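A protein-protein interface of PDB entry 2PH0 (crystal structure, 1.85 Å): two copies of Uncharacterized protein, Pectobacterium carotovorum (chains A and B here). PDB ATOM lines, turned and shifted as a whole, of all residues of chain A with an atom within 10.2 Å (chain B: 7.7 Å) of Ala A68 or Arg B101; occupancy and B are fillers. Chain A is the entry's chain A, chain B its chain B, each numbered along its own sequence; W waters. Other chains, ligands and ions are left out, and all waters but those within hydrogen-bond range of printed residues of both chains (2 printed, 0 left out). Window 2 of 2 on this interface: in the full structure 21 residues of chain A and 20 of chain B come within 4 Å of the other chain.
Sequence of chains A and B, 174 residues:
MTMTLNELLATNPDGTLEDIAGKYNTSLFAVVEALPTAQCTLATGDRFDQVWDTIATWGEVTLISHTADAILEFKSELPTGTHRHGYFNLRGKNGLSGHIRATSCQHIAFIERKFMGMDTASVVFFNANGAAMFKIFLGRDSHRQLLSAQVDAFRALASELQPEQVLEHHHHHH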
ATOM      1  N   THR A  16     -15.961  19.064  12.673  1.00  0.00           N
ATOM      2  CA  THR A  16     -14.719  18.443  12.224  1.00  0.00           C
ATOM      3  C   THR A  16     -14.746  18.338  10.703  1.00  0.00           C
ATOM      4  O   THR A  16     -15.815  18.175  10.108  1.00  0.00           O
ATOM      5  CB  THR A  16     -14.554  17.013  12.787  1.00  0.00           C
ATOM      6  OG1 THR A  16     -15.626  16.190  12.309  1.00  0.00           O
ATOM      7  CG2 THR A  16     -14.566  17.028  14.306  1.00  0.00           C
ATOM      8  N   LEU A  17     -13.580  18.431  10.072  1.00  0.00           N
ATOM      9  CA  LEU A  17     -13.524  18.308   8.624  1.00  0.00           C
ATOM     10  C   LEU A  17     -13.854  16.858   8.271  1.00  0.00           C
ATOM     11  O   LEU A  17     -14.274  16.557   7.158  1.00  0.00           O
ATOM     12  CB  LEU A  17     -12.140  18.707   8.106  1.00  0.00           C
ATOM     13  CG  LEU A  17     -11.861  20.208   8.276  1.00  0.00           C
ATOM     14  CD1 LEU A  17     -10.493  20.554   7.726  1.00  0.00           C
ATOM     15  CD2 LEU A  17     -12.955  21.011   7.548  1.00  0.00           C
ATOM     16  N   GLU A  18     -13.676  15.964   9.239  1.00  0.00           N
ATOM     17  CA  GLU A  18     -13.987  14.556   9.030  1.00  0.00           C
ATOM     18  C   GLU A  18     -15.480  14.367   8.798  1.00  0.00           C
ATOM     19  O   GLU A  18     -15.882  13.579   7.940  1.00  0.00           O
ATOM     20  CB  GLU A  18     -13.536  13.719  10.235  1.00  0.00           C
ATOM     21  CG  GLU A  18     -12.049  13.393  10.259  1.00  0.00           C
ATOM     22  CD  GLU A  18     -11.176  14.537  10.743  1.00  0.00           C
ATOM     23  OE1 GLU A  18     -11.715  15.608  11.088  1.00  0.00           O
ATOM     24  OE2 GLU A  18      -9.940  14.358  10.786  1.00  0.00           O
ATOM     25  N   ASP A  19     -16.302  15.084   9.558  1.00  0.00           N
ATOM     26  CA  ASP A  19     -17.754  14.988   9.401  1.00  0.00           C
ATOM     27  C   ASP A  19     -18.161  15.445   8.006  1.00  0.00           C
ATOM     28  O   ASP A  19     -19.057  14.864   7.386  1.00  0.00           O
ATOM     29  CB  ASP A  19     -18.467  15.837  10.459  1.00  0.00           C
ATOM     30  CG  ASP A  19     -18.520  15.152  11.818  1.00  0.00           C
ATOM     31  OD1 ASP A  19     -17.681  14.262  12.076  1.00  0.00           O
ATOM     32  OD2 ASP A  19     -19.398  15.511  12.632  1.00  0.00           O
ATOM     33  N   ILE A  20     -17.494  16.487   7.517  1.00  0.00           N
ATOM     34  CA  ILE A  20     -17.762  17.031   6.190  1.00  0.00           C
ATOM     35  C   ILE A  20     -17.336  16.027   5.112  1.00  0.00           C
ATOM     36  O   ILE A  20     -18.051  15.812   4.133  1.00  0.00           O
ATOM     37  CB  ILE A  20     -17.004  18.363   5.974  1.00  0.00           C
ATOM     38  CG1 ILE A  20     -17.493  19.409   6.981  1.00  0.00           C
ATOM     39  CG2 ILE A  20     -17.194  18.843   4.544  1.00  0.00           C
ATOM     40  CD1 ILE A  20     -16.719  20.719   6.938  1.00  0.00           C
ATOM     41  N   ALA A  21     -16.165  15.425   5.279  1.00  0.00           N
ATOM     42  CA  ALA A  21     -15.711  14.426   4.316  1.00  0.00           C
ATOM     43  C   ALA A  21     -16.761  13.314   4.278  1.00  0.00           C
ATOM     44  O   ALA A  21     -17.065  12.759   3.220  1.00  0.00           O
ATOM     45  CB  ALA A  21     -14.366  13.859   4.734  1.00  0.00           C
ATOM     46  N   GLY A  22     -17.315  12.998   5.445  1.00  0.00           N
ATOM     47  CA  GLY A  22     -18.329  11.963   5.533  1.00  0.00           C
ATOM     48  C   GLY A  22     -19.577  12.297   4.742  1.00  0.00           C
ATOM     49  O   GLY A  22     -20.058  11.482   3.954  1.00  0.00           O
ATOM     50  N   LYS A  23     -20.106  13.498   4.948  1.00  0.00           N
ATOM     51  CA  LYS A  23     -21.306  13.932   4.248  1.00  0.00           C
ATOM     52  C   LYS A  23     -21.148  13.891   2.730  1.00  0.00           C
ATOM     53  O   LYS A  23     -22.078  13.528   2.012  1.00  0.00           O
ATOM     54  CB  LYS A  23     -21.698  15.350   4.683  1.00  0.00           C
ATOM     55  CG  LYS A  23     -22.470  15.423   5.992  1.00  0.00           C
ATOM     56  CD  LYS A  23     -22.961  16.842   6.258  1.00  0.00           C
ATOM     57  CE  LYS A  23     -23.997  16.888   7.377  1.00  0.00           C
ATOM     58  NZ  LYS A  23     -23.455  16.447   8.693  1.00  0.00           N
ATOM     59  N   THR A  26     -16.237  11.508   0.769  1.00  0.00           N
ATOM     60  CA  THR A  26     -14.945  11.634   0.121  1.00  0.00           C
ATOM     61  C   THR A  26     -13.835  11.581   1.165  1.00  0.00           C
ATOM     62  O   THR A  26     -14.088  11.280   2.328  1.00  0.00           O
ATOM     63  CB  THR A  26     -14.861  12.943  -0.684  1.00  0.00           C
ATOM     64  OG1 THR A  26     -13.678  12.936  -1.490  1.00  0.00           O
ATOM     65  CG2 THR A  26     -14.846  14.138   0.244  1.00  0.00           C
ATOM     66  N   LEU A  28     -10.610  13.062   3.546  1.00  0.00           N
ATOM     67  CA  LEU A  28     -10.345  14.269   4.312  1.00  0.00           C
ATOM     68  C   LEU A  28      -9.520  15.215   3.436  1.00  0.00           C
ATOM     69  O   LEU A  28      -9.730  16.430   3.445  1.00  0.00           O
ATOM     70  CB  LEU A  28      -9.551  13.933   5.576  1.00  0.00           C
ATOM     71  CG  LEU A  28      -9.118  15.119   6.442  1.00  0.00           C
ATOM     72  CD1 LEU A  28     -10.345  15.863   6.963  1.00  0.00           C
ATOM     73  CD2 LEU A  28      -8.261  14.614   7.591  1.00  0.00           C
ATOM     74  N   SER A  65      -4.543  10.994  16.613  1.00  0.00           N
ATOM     75  CA  SER A  65      -4.876   9.947  15.657  1.00  0.00           C
ATOM     76  C   SER A  65      -6.386  10.114  15.562  1.00  0.00           C
ATOM     77  O   SER A  65      -7.086  10.015  16.570  1.00  0.00           O
ATOM     78  CB  SER A  65      -4.547   8.557  16.207  1.00  0.00           C
ATOM     79  OG  SER A  65      -5.301   7.588  15.507  1.00  0.00           O
ATOM     80  N   HIS A  66      -6.889  10.379  14.363  1.00  0.00           N
ATOM     81  CA  HIS A  66      -8.313  10.599  14.183  1.00  0.00           C
ATOM     82  C   HIS A  66      -8.897   9.685  13.120  1.00  0.00           C
ATOM     83  O   HIS A  66      -8.574   9.811  11.939  1.00  0.00           O
ATOM     84  CB  HIS A  66      -8.552  12.068  13.809  1.00  0.00           C
ATOM     85  CG  HIS A  66      -9.992  12.472  13.806  1.00  0.00           C
ATOM     86  ND1 HIS A  66     -10.397  13.756  14.106  1.00  0.00           N
ATOM     87  CD2 HIS A  66     -11.121  11.781  13.522  1.00  0.00           C
ATOM     88  CE1 HIS A  66     -11.711  13.836  14.009  1.00  0.00           C
ATOM     89  NE2 HIS A  66     -12.175  12.651  13.655  1.00  0.00           N
ATOM     90  N   THR A  67      -9.742   8.754  13.555  1.00  0.00           N
ATOM     91  CA  THR A  67     -10.406   7.820  12.644  1.00  0.00           C
ATOM     92  C   THR A  67     -11.911   7.903  12.887  1.00  0.00           C
ATOM     93  O   THR A  67     -12.372   8.644  13.752  1.00  0.00           O
ATOM     94  CB  THR A  67      -9.966   6.355  12.881  1.00  0.00           C
ATOM     95  OG1 THR A  67     -10.560   5.856  14.087  1.00  0.00           O
ATOM     96  CG2 THR A  67      -8.455   6.264  12.996  1.00  0.00           C
ATOM     97  N   ALA A  68     -12.675   7.143  12.113  1.00  0.00           N
ATOM     98  CA  ALA A  68     -14.122   7.129  12.253  1.00  0.00           C
ATOM     99  C   ALA A  68     -14.537   6.491  13.573  1.00  0.00           C
ATOM    100  O   ALA A  68     -15.658   6.686  14.029  1.00  0.00           O
ATOM    101  CB  ALA A  68     -14.743   6.362  11.096  1.00  0.00           C
ATOM    102  N   ASP A  69     -13.633   5.734  14.189  1.00  0.00           N
ATOM    103  CA  ASP A  69     -13.951   5.058  15.440  1.00  0.00           C
ATOM    104  C   ASP A  69     -13.395   5.750  16.677  1.00  0.00           C
ATOM    105  O   ASP A  69     -13.944   5.610  17.767  1.00  0.00           O
ATOM    106  CB  ASP A  69     -13.430   3.614  15.427  1.00  0.00           C
ATOM    107  CG  ASP A  69     -13.766   2.870  14.149  1.00  0.00           C
ATOM    108  OD1 ASP A  69     -14.953   2.809  13.773  1.00  0.00           O
ATOM    109  OD2 ASP A  69     -12.830   2.330  13.520  1.00  0.00           O
ATOM    110  N   ALA A  70     -12.304   6.490  16.528  1.00  0.00           N
ATOM    111  CA  ALA A  70     -11.734   7.124  17.696  1.00  0.00           C
ATOM    112  C   ALA A  70     -10.806   8.279  17.414  1.00  0.00           C
ATOM    113  O   ALA A  70     -10.156   8.342  16.376  1.00  0.00           O
ATOM    114  CB  ALA A  70     -10.990   6.085  18.528  1.00  0.00           C
ATOM    115  N   ILE A  71     -10.764   9.190  18.376  1.00  0.00           N
ATOM    116  CA  ILE A  71      -9.892  10.342  18.329  1.00  0.00           C
ATOM    117  C   ILE A  71      -9.022  10.198  19.575  1.00  0.00           C
ATOM    118  O   ILE A  71      -9.508  10.327  20.694  1.00  0.00           O
ATOM    119  CB  ILE A  71     -10.686  11.650  18.424  1.00  0.00           C
ATOM    120  CG1 ILE A  71     -11.700  11.729  17.284  1.00  0.00           C
ATOM    121  CG2 ILE A  71      -9.735  12.823  18.371  1.00  0.00           C
ATOM    122  CD1 ILE A  71     -12.638  12.913  17.382  1.00  0.00           C
ATOM    123  N   LEU A  72      -7.744   9.904  19.374  1.00  0.00           N
ATOM    124  CA  LEU A  72      -6.810   9.731  20.478  1.00  0.00           C
ATOM    125  C   LEU A  72      -5.864  10.914  20.468  1.00  0.00           C
ATOM    126  O   LEU A  72      -5.237  11.203  19.443  1.00  0.00           O
ATOM    127  CB  LEU A  72      -6.048   8.418  20.300  1.00  0.00           C
ATOM    128  CG  LEU A  72      -7.009   7.229  20.178  1.00  0.00           C
ATOM    129  CD1 LEU A  72      -6.246   5.962  19.818  1.00  0.00           C
ATOM    130  CD2 LEU A  72      -7.789   7.071  21.477  1.00  0.00           C
ATOM    131  N   ALA A 131      -6.102  10.183   3.425  1.00  0.00           N
ATOM    132  CA  ALA A 131      -6.498  10.059   4.816  1.00  0.00           C
ATOM    133  C   ALA A 131      -5.432  10.696   5.703  1.00  0.00           C
ATOM    134  O   ALA A 131      -4.288  10.875   5.283  1.00  0.00           O
ATOM    135  CB  ALA A 131      -6.676   8.582   5.181  1.00  0.00           C
ATOM    136  N   ALA A 132      -5.810  11.055   6.925  1.00  0.00           N
ATOM    137  CA  ALA A 132      -4.853  11.643   7.854  1.00  0.00           C
ATOM    138  C   ALA A 132      -4.083  10.533   8.562  1.00  0.00           C
ATOM    139  O   ALA A 132      -4.676   9.685   9.232  1.00  0.00           O
ATOM    140  CB  ALA A 132      -5.585  12.512   8.887  1.00  0.00           C
ATOM    141  N   LYS A 135      -2.333  13.976  13.091  1.00  0.00           N
ATOM    142  CA  LYS A 135      -2.436  15.433  13.058  1.00  0.00           C
ATOM    143  C   LYS A 135      -1.700  16.003  14.256  1.00  0.00           C
ATOM    144  O   LYS A 135      -1.455  15.299  15.233  1.00  0.00           O
ATOM    145  CB  LYS A 135      -3.886  15.883  13.177  1.00  0.00           C
ATOM    146  CG  LYS A 135      -4.873  15.217  12.258  1.00  0.00           C
ATOM    147  CD  LYS A 135      -6.237  15.852  12.496  1.00  0.00           C
ATOM    148  CE  LYS A 135      -7.257  15.412  11.473  1.00  0.00           C
ATOM    149  NZ  LYS A 135      -8.528  16.147  11.688  1.00  0.00           N
ATOM    150  N   PHE B  48     -17.553  -3.010  26.536  1.00  0.00           N
ATOM    151  CA  PHE B  48     -16.574  -1.926  26.497  1.00  0.00           C
ATOM    152  C   PHE B  48     -16.422  -1.080  27.758  1.00  0.00           C
ATOM    153  O   PHE B  48     -15.307  -0.884  28.241  1.00  0.00           O
ATOM    154  CB  PHE B  48     -16.859  -1.009  25.303  1.00  0.00           C
ATOM    155  CG  PHE B  48     -15.883   0.128  25.165  1.00  0.00           C
ATOM    156  CD1 PHE B  48     -16.073   1.318  25.868  1.00  0.00           C
ATOM    157  CD2 PHE B  48     -14.762   0.002  24.349  1.00  0.00           C
ATOM    158  CE1 PHE B  48     -15.161   2.366  25.760  1.00  0.00           C
ATOM    159  CE2 PHE B  48     -13.843   1.044  24.234  1.00  0.00           C
ATOM    160  CZ  PHE B  48     -14.045   2.227  24.941  1.00  0.00           C
ATOM    161  N   HIS B  83     -20.135   9.313  28.667  1.00  0.00           N
ATOM    162  CA  HIS B  83     -20.821   9.234  27.379  1.00  0.00           C
ATOM    163  C   HIS B  83     -21.691  10.459  27.108  1.00  0.00           C
ATOM    164  O   HIS B  83     -22.396  10.944  27.992  1.00  0.00           O
ATOM    165  CB  HIS B  83     -21.709   7.983  27.326  1.00  0.00           C
ATOM    166  CG  HIS B  83     -20.948   6.692  27.285  1.00  0.00           C
ATOM    167  ND1 HIS B  83     -20.258   6.270  26.170  1.00  0.00           N
ATOM    168  CD2 HIS B  83     -20.797   5.716  28.213  1.00  0.00           C
ATOM    169  CE1 HIS B  83     -19.717   5.089  26.411  1.00  0.00           C
ATOM    170  NE2 HIS B  83     -20.028   4.731  27.643  1.00  0.00           N
ATOM    171  N   HIS B  85     -23.585  12.408  23.378  1.00  0.00           N
ATOM    172  CA  HIS B  85     -23.714  12.601  21.940  1.00  0.00           C
ATOM    173  C   HIS B  85     -23.170  11.463  21.078  1.00  0.00           C
ATOM    174  O   HIS B  85     -22.789  11.680  19.930  1.00  0.00           O
ATOM    175  CB  HIS B  85     -23.047  13.919  21.538  1.00  0.00           C
ATOM    176  CG  HIS B  85     -23.640  15.118  22.210  1.00  0.00           C
ATOM    177  ND1 HIS B  85     -22.872  16.099  22.799  1.00  0.00           N
ATOM    178  CD2 HIS B  85     -24.930  15.484  22.403  1.00  0.00           C
ATOM    179  CE1 HIS B  85     -23.662  17.017  23.327  1.00  0.00           C
ATOM    180  NE2 HIS B  85     -24.916  16.667  23.101  1.00  0.00           N
ATOM    181  N   GLY B  86     -23.139  10.253  21.621  1.00  0.00           N
ATOM    182  CA  GLY B  86     -22.657   9.133  20.837  1.00  0.00           C
ATOM    183  C   GLY B  86     -21.181   8.839  21.000  1.00  0.00           C
ATOM    184  O   GLY B  86     -20.649   7.942  20.348  1.00  0.00           O
ATOM    185  N   TYR B  87     -20.516   9.588  21.870  1.00  0.00           N
ATOM    186  CA  TYR B  87     -19.097   9.380  22.113  1.00  0.00           C
ATOM    187  C   TYR B  87     -18.754   9.187  23.578  1.00  0.00           C
ATOM    188  O   TYR B  87     -19.419   9.725  24.462  1.00  0.00           O
ATOM    189  CB  TYR B  87     -18.275  10.557  21.573  1.00  0.00           C
ATOM    190  CG  TYR B  87     -17.973  10.462  20.099  1.00  0.00           C
ATOM    191  CD1 TYR B  87     -18.952  10.736  19.146  1.00  0.00           C
ATOM    192  CD2 TYR B  87     -16.713  10.050  19.657  1.00  0.00           C
ATOM    193  CE1 TYR B  87     -18.687  10.601  17.782  1.00  0.00           C
ATOM    194  CE2 TYR B  87     -16.436   9.909  18.300  1.00  0.00           C
ATOM    195  CZ  TYR B  87     -17.428  10.184  17.368  1.00  0.00           C
ATOM    196  OH  TYR B  87     -17.166  10.027  16.028  1.00  0.00           O
ATOM    197  N   PHE B  88     -17.722   8.383  23.818  1.00  0.00           N
ATOM    198  CA  PHE B  88     -17.210   8.138  25.161  1.00  0.00           C
ATOM    199  C   PHE B  88     -16.072   9.153  25.239  1.00  0.00           C
ATOM    200  O   PHE B  88     -15.028   8.995  24.600  1.00  0.00           O
ATOM    201  CB  PHE B  88     -16.677   6.707  25.277  1.00  0.00           C
ATOM    202  CG  PHE B  88     -16.100   6.372  26.633  1.00  0.00           C
ATOM    203  CD1 PHE B  88     -16.913   6.336  27.765  1.00  0.00           C
ATOM    204  CD2 PHE B  88     -14.750   6.062  26.771  1.00  0.00           C
ATOM    205  CE1 PHE B  88     -16.390   5.989  29.016  1.00  0.00           C
ATOM    206  CE2 PHE B  88     -14.215   5.714  28.016  1.00  0.00           C
ATOM    207  CZ  PHE B  88     -15.038   5.678  29.141  1.00  0.00           C
ATOM    208  N   ASN B  89     -16.288  10.213  26.008  1.00  0.00           N
ATOM    209  CA  ASN B  89     -15.312  11.286  26.121  1.00  0.00           C
ATOM    210  C   ASN B  89     -14.389  11.124  27.319  1.00  0.00           C
ATOM    211  O   ASN B  89     -14.846  10.983  28.452  1.00  0.00           O
ATOM    212  CB  ASN B  89     -16.062  12.617  26.186  1.00  0.00           C
ATOM    213  CG  ASN B  89     -17.048  12.770  25.044  1.00  0.00           C
ATOM    214  OD1 ASN B  89     -16.659  12.794  23.875  1.00  0.00           O
ATOM    215  ND2 ASN B  89     -18.333  12.849  25.374  1.00  0.00           N
ATOM    216  N   GLY B  98      -9.186  12.208  24.546  1.00  0.00           N
ATOM    217  CA  GLY B  98      -9.789  11.815  23.288  1.00  0.00           C
ATOM    218  C   GLY B  98     -11.259  11.469  23.371  1.00  0.00           C
ATOM    219  O   GLY B  98     -11.910  11.637  24.413  1.00  0.00           O
ATOM    220  N   HIS B  99     -11.774  10.953  22.261  1.00  0.00           N
ATOM    221  CA  HIS B  99     -13.178  10.598  22.137  1.00  0.00           C
ATOM    222  C   HIS B  99     -13.274   9.282  21.390  1.00  0.00           C
ATOM    223  O   HIS B  99     -12.741   9.155  20.291  1.00  0.00           O
ATOM    224  CB  HIS B  99     -13.893  11.686  21.339  1.00  0.00           C
ATOM    225  CG  HIS B  99     -13.622  13.071  21.841  1.00  0.00           C
ATOM    226  ND1 HIS B  99     -14.307  13.623  22.903  1.00  0.00           N
ATOM    227  CD2 HIS B  99     -12.698  13.989  21.470  1.00  0.00           C
ATOM    228  CE1 HIS B  99     -13.815  14.821  23.164  1.00  0.00           C
ATOM    229  NE2 HIS B  99     -12.839  15.067  22.310  1.00  0.00           N
ATOM    230  N   ILE B 100     -13.945   8.304  21.989  1.00  0.00           N
ATOM    231  CA  ILE B 100     -14.106   6.997  21.358  1.00  0.00           C
ATOM    232  C   ILE B 100     -15.572   6.802  20.974  1.00  0.00           C
ATOM    233  O   ILE B 100     -16.463   6.923  21.820  1.00  0.00           O
ATOM    234  CB  ILE B 100     -13.648   5.883  22.322  1.00  0.00           C
ATOM    235  CG1 ILE B 100     -12.172   6.098  22.668  1.00  0.00           C
ATOM    236  CG2 ILE B 100     -13.875   4.512  21.695  1.00  0.00           C
ATOM    237  CD1 ILE B 100     -11.674   5.302  23.869  1.00  0.00           C
ATOM    238  N   ARG B 101     -15.826   6.504  19.704  1.00  0.00           N
ATOM    239  CA  ARG B 101     -17.199   6.322  19.240  1.00  0.00           C
ATOM    240  C   ARG B 101     -17.824   5.068  19.841  1.00  0.00           C
ATOM    241  O   ARG B 101     -17.332   3.953  19.640  1.00  0.00           O
ATOM    242  CB  ARG B 101     -17.252   6.266  17.714  1.00  0.00           C
ATOM    243  CG  ARG B 101     -18.680   6.235  17.174  1.00  0.00           C
ATOM    244  CD  ARG B 101     -18.717   6.238  15.655  1.00  0.00           C
ATOM    245  NE  ARG B 101     -18.122   7.447  15.095  1.00  0.00           N
ATOM    246  CZ  ARG B 101     -18.196   7.790  13.812  1.00  0.00           C
ATOM    247  NH1 ARG B 101     -18.843   7.014  12.953  1.00  0.00           N
ATOM    248  NH2 ARG B 101     -17.621   8.908  13.387  1.00  0.00           N
ATOM    249  N   ALA B 102     -18.927   5.276  20.562  1.00  0.00           N
ATOM    250  CA  ALA B 102     -19.658   4.220  21.273  1.00  0.00           C
ATOM    251  C   ALA B 102     -20.064   2.969  20.500  1.00  0.00           C
ATOM    252  O   ALA B 102     -19.830   1.854  20.955  1.00  0.00           O
ATOM    253  CB  ALA B 102     -20.893   4.825  21.941  1.00  0.00           C
ATOM    254  N   THR B 103     -20.687   3.151  19.344  1.00  0.00           N
ATOM    255  CA  THR B 103     -21.144   2.024  18.535  1.00  0.00           C
ATOM    256  C   THR B 103     -20.034   1.292  17.781  1.00  0.00           C
ATOM    257  O   THR B 103     -20.268   0.237  17.189  1.00  0.00           O
ATOM    258  CB  THR B 103     -22.172   2.495  17.481  1.00  0.00           C
ATOM    259  OG1 THR B 103     -22.721   1.358  16.802  1.00  0.00           O
ATOM    260  CG2 THR B 103     -21.490   3.407  16.450  1.00  0.00           C
ATOM    261  N   SER B 104     -18.828   1.840  17.802  1.00  0.00           N
ATOM    262  CA  SER B 104     -17.738   1.247  17.040  1.00  0.00           C
ATOM    263  C   SER B 104     -17.164  -0.087  17.501  1.00  0.00           C
ATOM    264  O   SER B 104     -16.872  -0.952  16.670  1.00  0.00           O
ATOM    265  CB  SER B 104     -16.601   2.261  16.897  1.00  0.00           C
ATOM    266  OG  SER B 104     -16.991   3.316  16.039  1.00  0.00           O
ATOM    267  N   CYS B 105     -17.012  -0.272  18.805  1.00  0.00           N
ATOM    268  CA  CYS B 105     -16.419  -1.521  19.289  1.00  0.00           C
ATOM    269  C   CYS B 105     -17.347  -2.728  19.209  1.00  0.00           C
ATOM    270  O   CYS B 105     -18.389  -2.769  19.855  1.00  0.00           O
ATOM    271  CB  CYS B 105     -15.912  -1.349  20.716  1.00  0.00           C
ATOM    272  SG  CYS B 105     -14.990  -2.801  21.299  1.00  0.00           S
ATOM    273  N   ASN B 127     -13.280  -2.877  15.623  1.00  0.00           N
ATOM    274  CA  ASN B 127     -14.494  -2.304  15.055  1.00  0.00           C
ATOM    275  C   ASN B 127     -15.178  -3.391  14.212  1.00  0.00           C
ATOM    276  O   ASN B 127     -14.716  -4.536  14.170  1.00  0.00           O
ATOM    277  CB  ASN B 127     -14.179  -1.065  14.191  1.00  0.00           C
ATOM    278  CG  ASN B 127     -13.237  -1.364  13.036  1.00  0.00           C
ATOM    279  OD1 ASN B 127     -13.121  -2.504  12.586  1.00  0.00           O
ATOM    280  ND2 ASN B 127     -12.575  -0.325  12.533  1.00  0.00           N
ATOM    281  N   MET B 133      -9.032  -0.723  16.877  1.00  0.00           N
ATOM    282  CA  MET B 133      -9.259   0.704  17.083  1.00  0.00           C
ATOM    283  C   MET B 133      -8.060   1.203  17.883  1.00  0.00           C
ATOM    284  O   MET B 133      -7.532   2.293  17.645  1.00  0.00           O
ATOM    285  CB  MET B 133     -10.567   0.904  17.840  1.00  0.00           C
ATOM    286  CG  MET B 133     -11.775   0.491  17.018  1.00  0.00           C
ATOM    287  SD  MET B 133     -13.382   0.304  18.055  1.00  0.00           S
ATOM    288  CE  MET B 133     -13.240   1.924  19.101  1.00  0.00           C
ATOM    289  N   PHE B 134      -7.629   0.378  18.831  1.00  0.00           N
ATOM    290  CA  PHE B 134      -6.465   0.657  19.655  1.00  0.00           C
ATOM    291  C   PHE B 134      -6.177  -0.575  20.499  1.00  0.00           C
ATOM    292  O   PHE B 134      -6.986  -1.504  20.554  1.00  0.00           O
ATOM    293  CB  PHE B 134      -6.663   1.893  20.561  1.00  0.00           C
ATOM    294  CG  PHE B 134      -7.989   1.940  21.264  1.00  0.00           C
ATOM    295  CD1 PHE B 134      -9.082   2.556  20.667  1.00  0.00           C
ATOM    296  CD2 PHE B 134      -8.152   1.354  22.516  1.00  0.00           C
ATOM    297  CE1 PHE B 134     -10.322   2.585  21.304  1.00  0.00           C
ATOM    298  CE2 PHE B 134      -9.389   1.378  23.161  1.00  0.00           C
ATOM    299  CZ  PHE B 134     -10.475   1.992  22.553  1.00  0.00           C
HETATM  300  O   HOH W   1      -8.523   4.414  16.225  1.00  0.00           O
HETATM  301  O   HOH W   2     -14.505   9.791  15.217  1.00  0.00           O
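The side-chain hydroxyl (OG) of Ser B104 sits at hydrogen-bond distance from the side-chain carboxylate (OD1) of Asp A69 (3.1 Å).
OD2 of Asp A69 is in hydrogen-bond range of ND2 of Asn B127 (2.8 Å).
The guanidinium group (NE) of Arg B101 lies close to the backbone carbonyl oxygen (O) of Ala A68 (2.8 Å).
The backbone carbonyl oxygen (O) of Asp A69 lies within hydrogen-bond range of the backbone NH (N) of Arg B101 (2.8 Å).
The backbone carbonyl oxygen of His B99 lies within hydrogen-bond range of the backbone NH of Ile A71, at 2.8 Å.
N of Phe B88 sits at hydrogen-bond distance from O of Ile B100, 2.8 Å away.
OG1 of Thr A67 sits close to N of Asp A69.
The side-chain hydroxyl of Tyr B87 is in hydrogen-bond range of the guanidinium group of Arg B101 (2.9 Å).
OG1 of Thr A67 lies within hydrogen-bond range of N of Ala A70 (3.1 Å).
The side-chain amide oxygen (OD1) of Asn B89 is in hydrogen-bond range of a ring nitrogen (ND1) of His B99 (2.7 Å).
The side-chain sulfur (SD) of Met B133 lies within hydrogen-bond range of the backbone NH (N) of Cys B105 (3.8 Å).
Ile B100 touches Asp A69 (C to O, 3.8 Å).
Met B133 touches Asp A69.
O of His B99 touches CA of Ala A70, 3.4 Å away.
Gly B98 touches Ile A71.
Ser A65 touches none of the printed residues of chain B.
Ala A68 touches just one residue of chain B: Arg B101.
Printed residues of chain B within 4 Å of Asp A69: Ile B100 (3.8 Å), Arg B101 (2.8 Å), Ser B104 (3.1 Å), Asn B127 (2.8 Å) and Met B133 (3.9 Å).
Phe B48 touches none of the printed residues of chain A.
Of the printed residues of chain A, Gly B98 touches Ile A71.
Of chain A, only Asp A69 comes within 4 Å of Ile B100.
Arg B101 touches just these residues of chain A: Ala A68 (2.8 Å) and Asp A69 (2.8 Å).
No residue of chain A comes within 4 Å of Ala B102.
Printed residues of chain A within 4 Å of Ser B104: Asp A69 (3.1 Å).
Of the printed residues of chain A, Met B133 touches Asp A69.
The nearest residue of chain A that does not touch Arg B101 is Ala A70 (4.6 Å).
The nearest printed residue of chain B that does not touch Asp A69 is His B99 (4.5 Å).
Of the 18 printed residues of chain B, 7 touch a printed residue of chain A.
Hydrophobic or aromatic side chains of chain B that line the printed part of chain A: Met B133.
Among the printed residues, no Asp or Glu carboxylate lies within 4 Å of a Lys or Arg side-chain nitrogen of the other chain.
No position is printed for both chains.
Of the 9 pairs that touch across the chains among the printed residues, none has its exchanged pair printed and touching as well.
Water W1 lies within hydrogen-bond range of O of Met B133 (2.7 Å) and OG1 of Thr A67 (3.3 Å).
Water W2 lies within hydrogen-bond range of OH of Tyr B87 (2.8 Å) and O of Thr A67 (2.8 Å).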
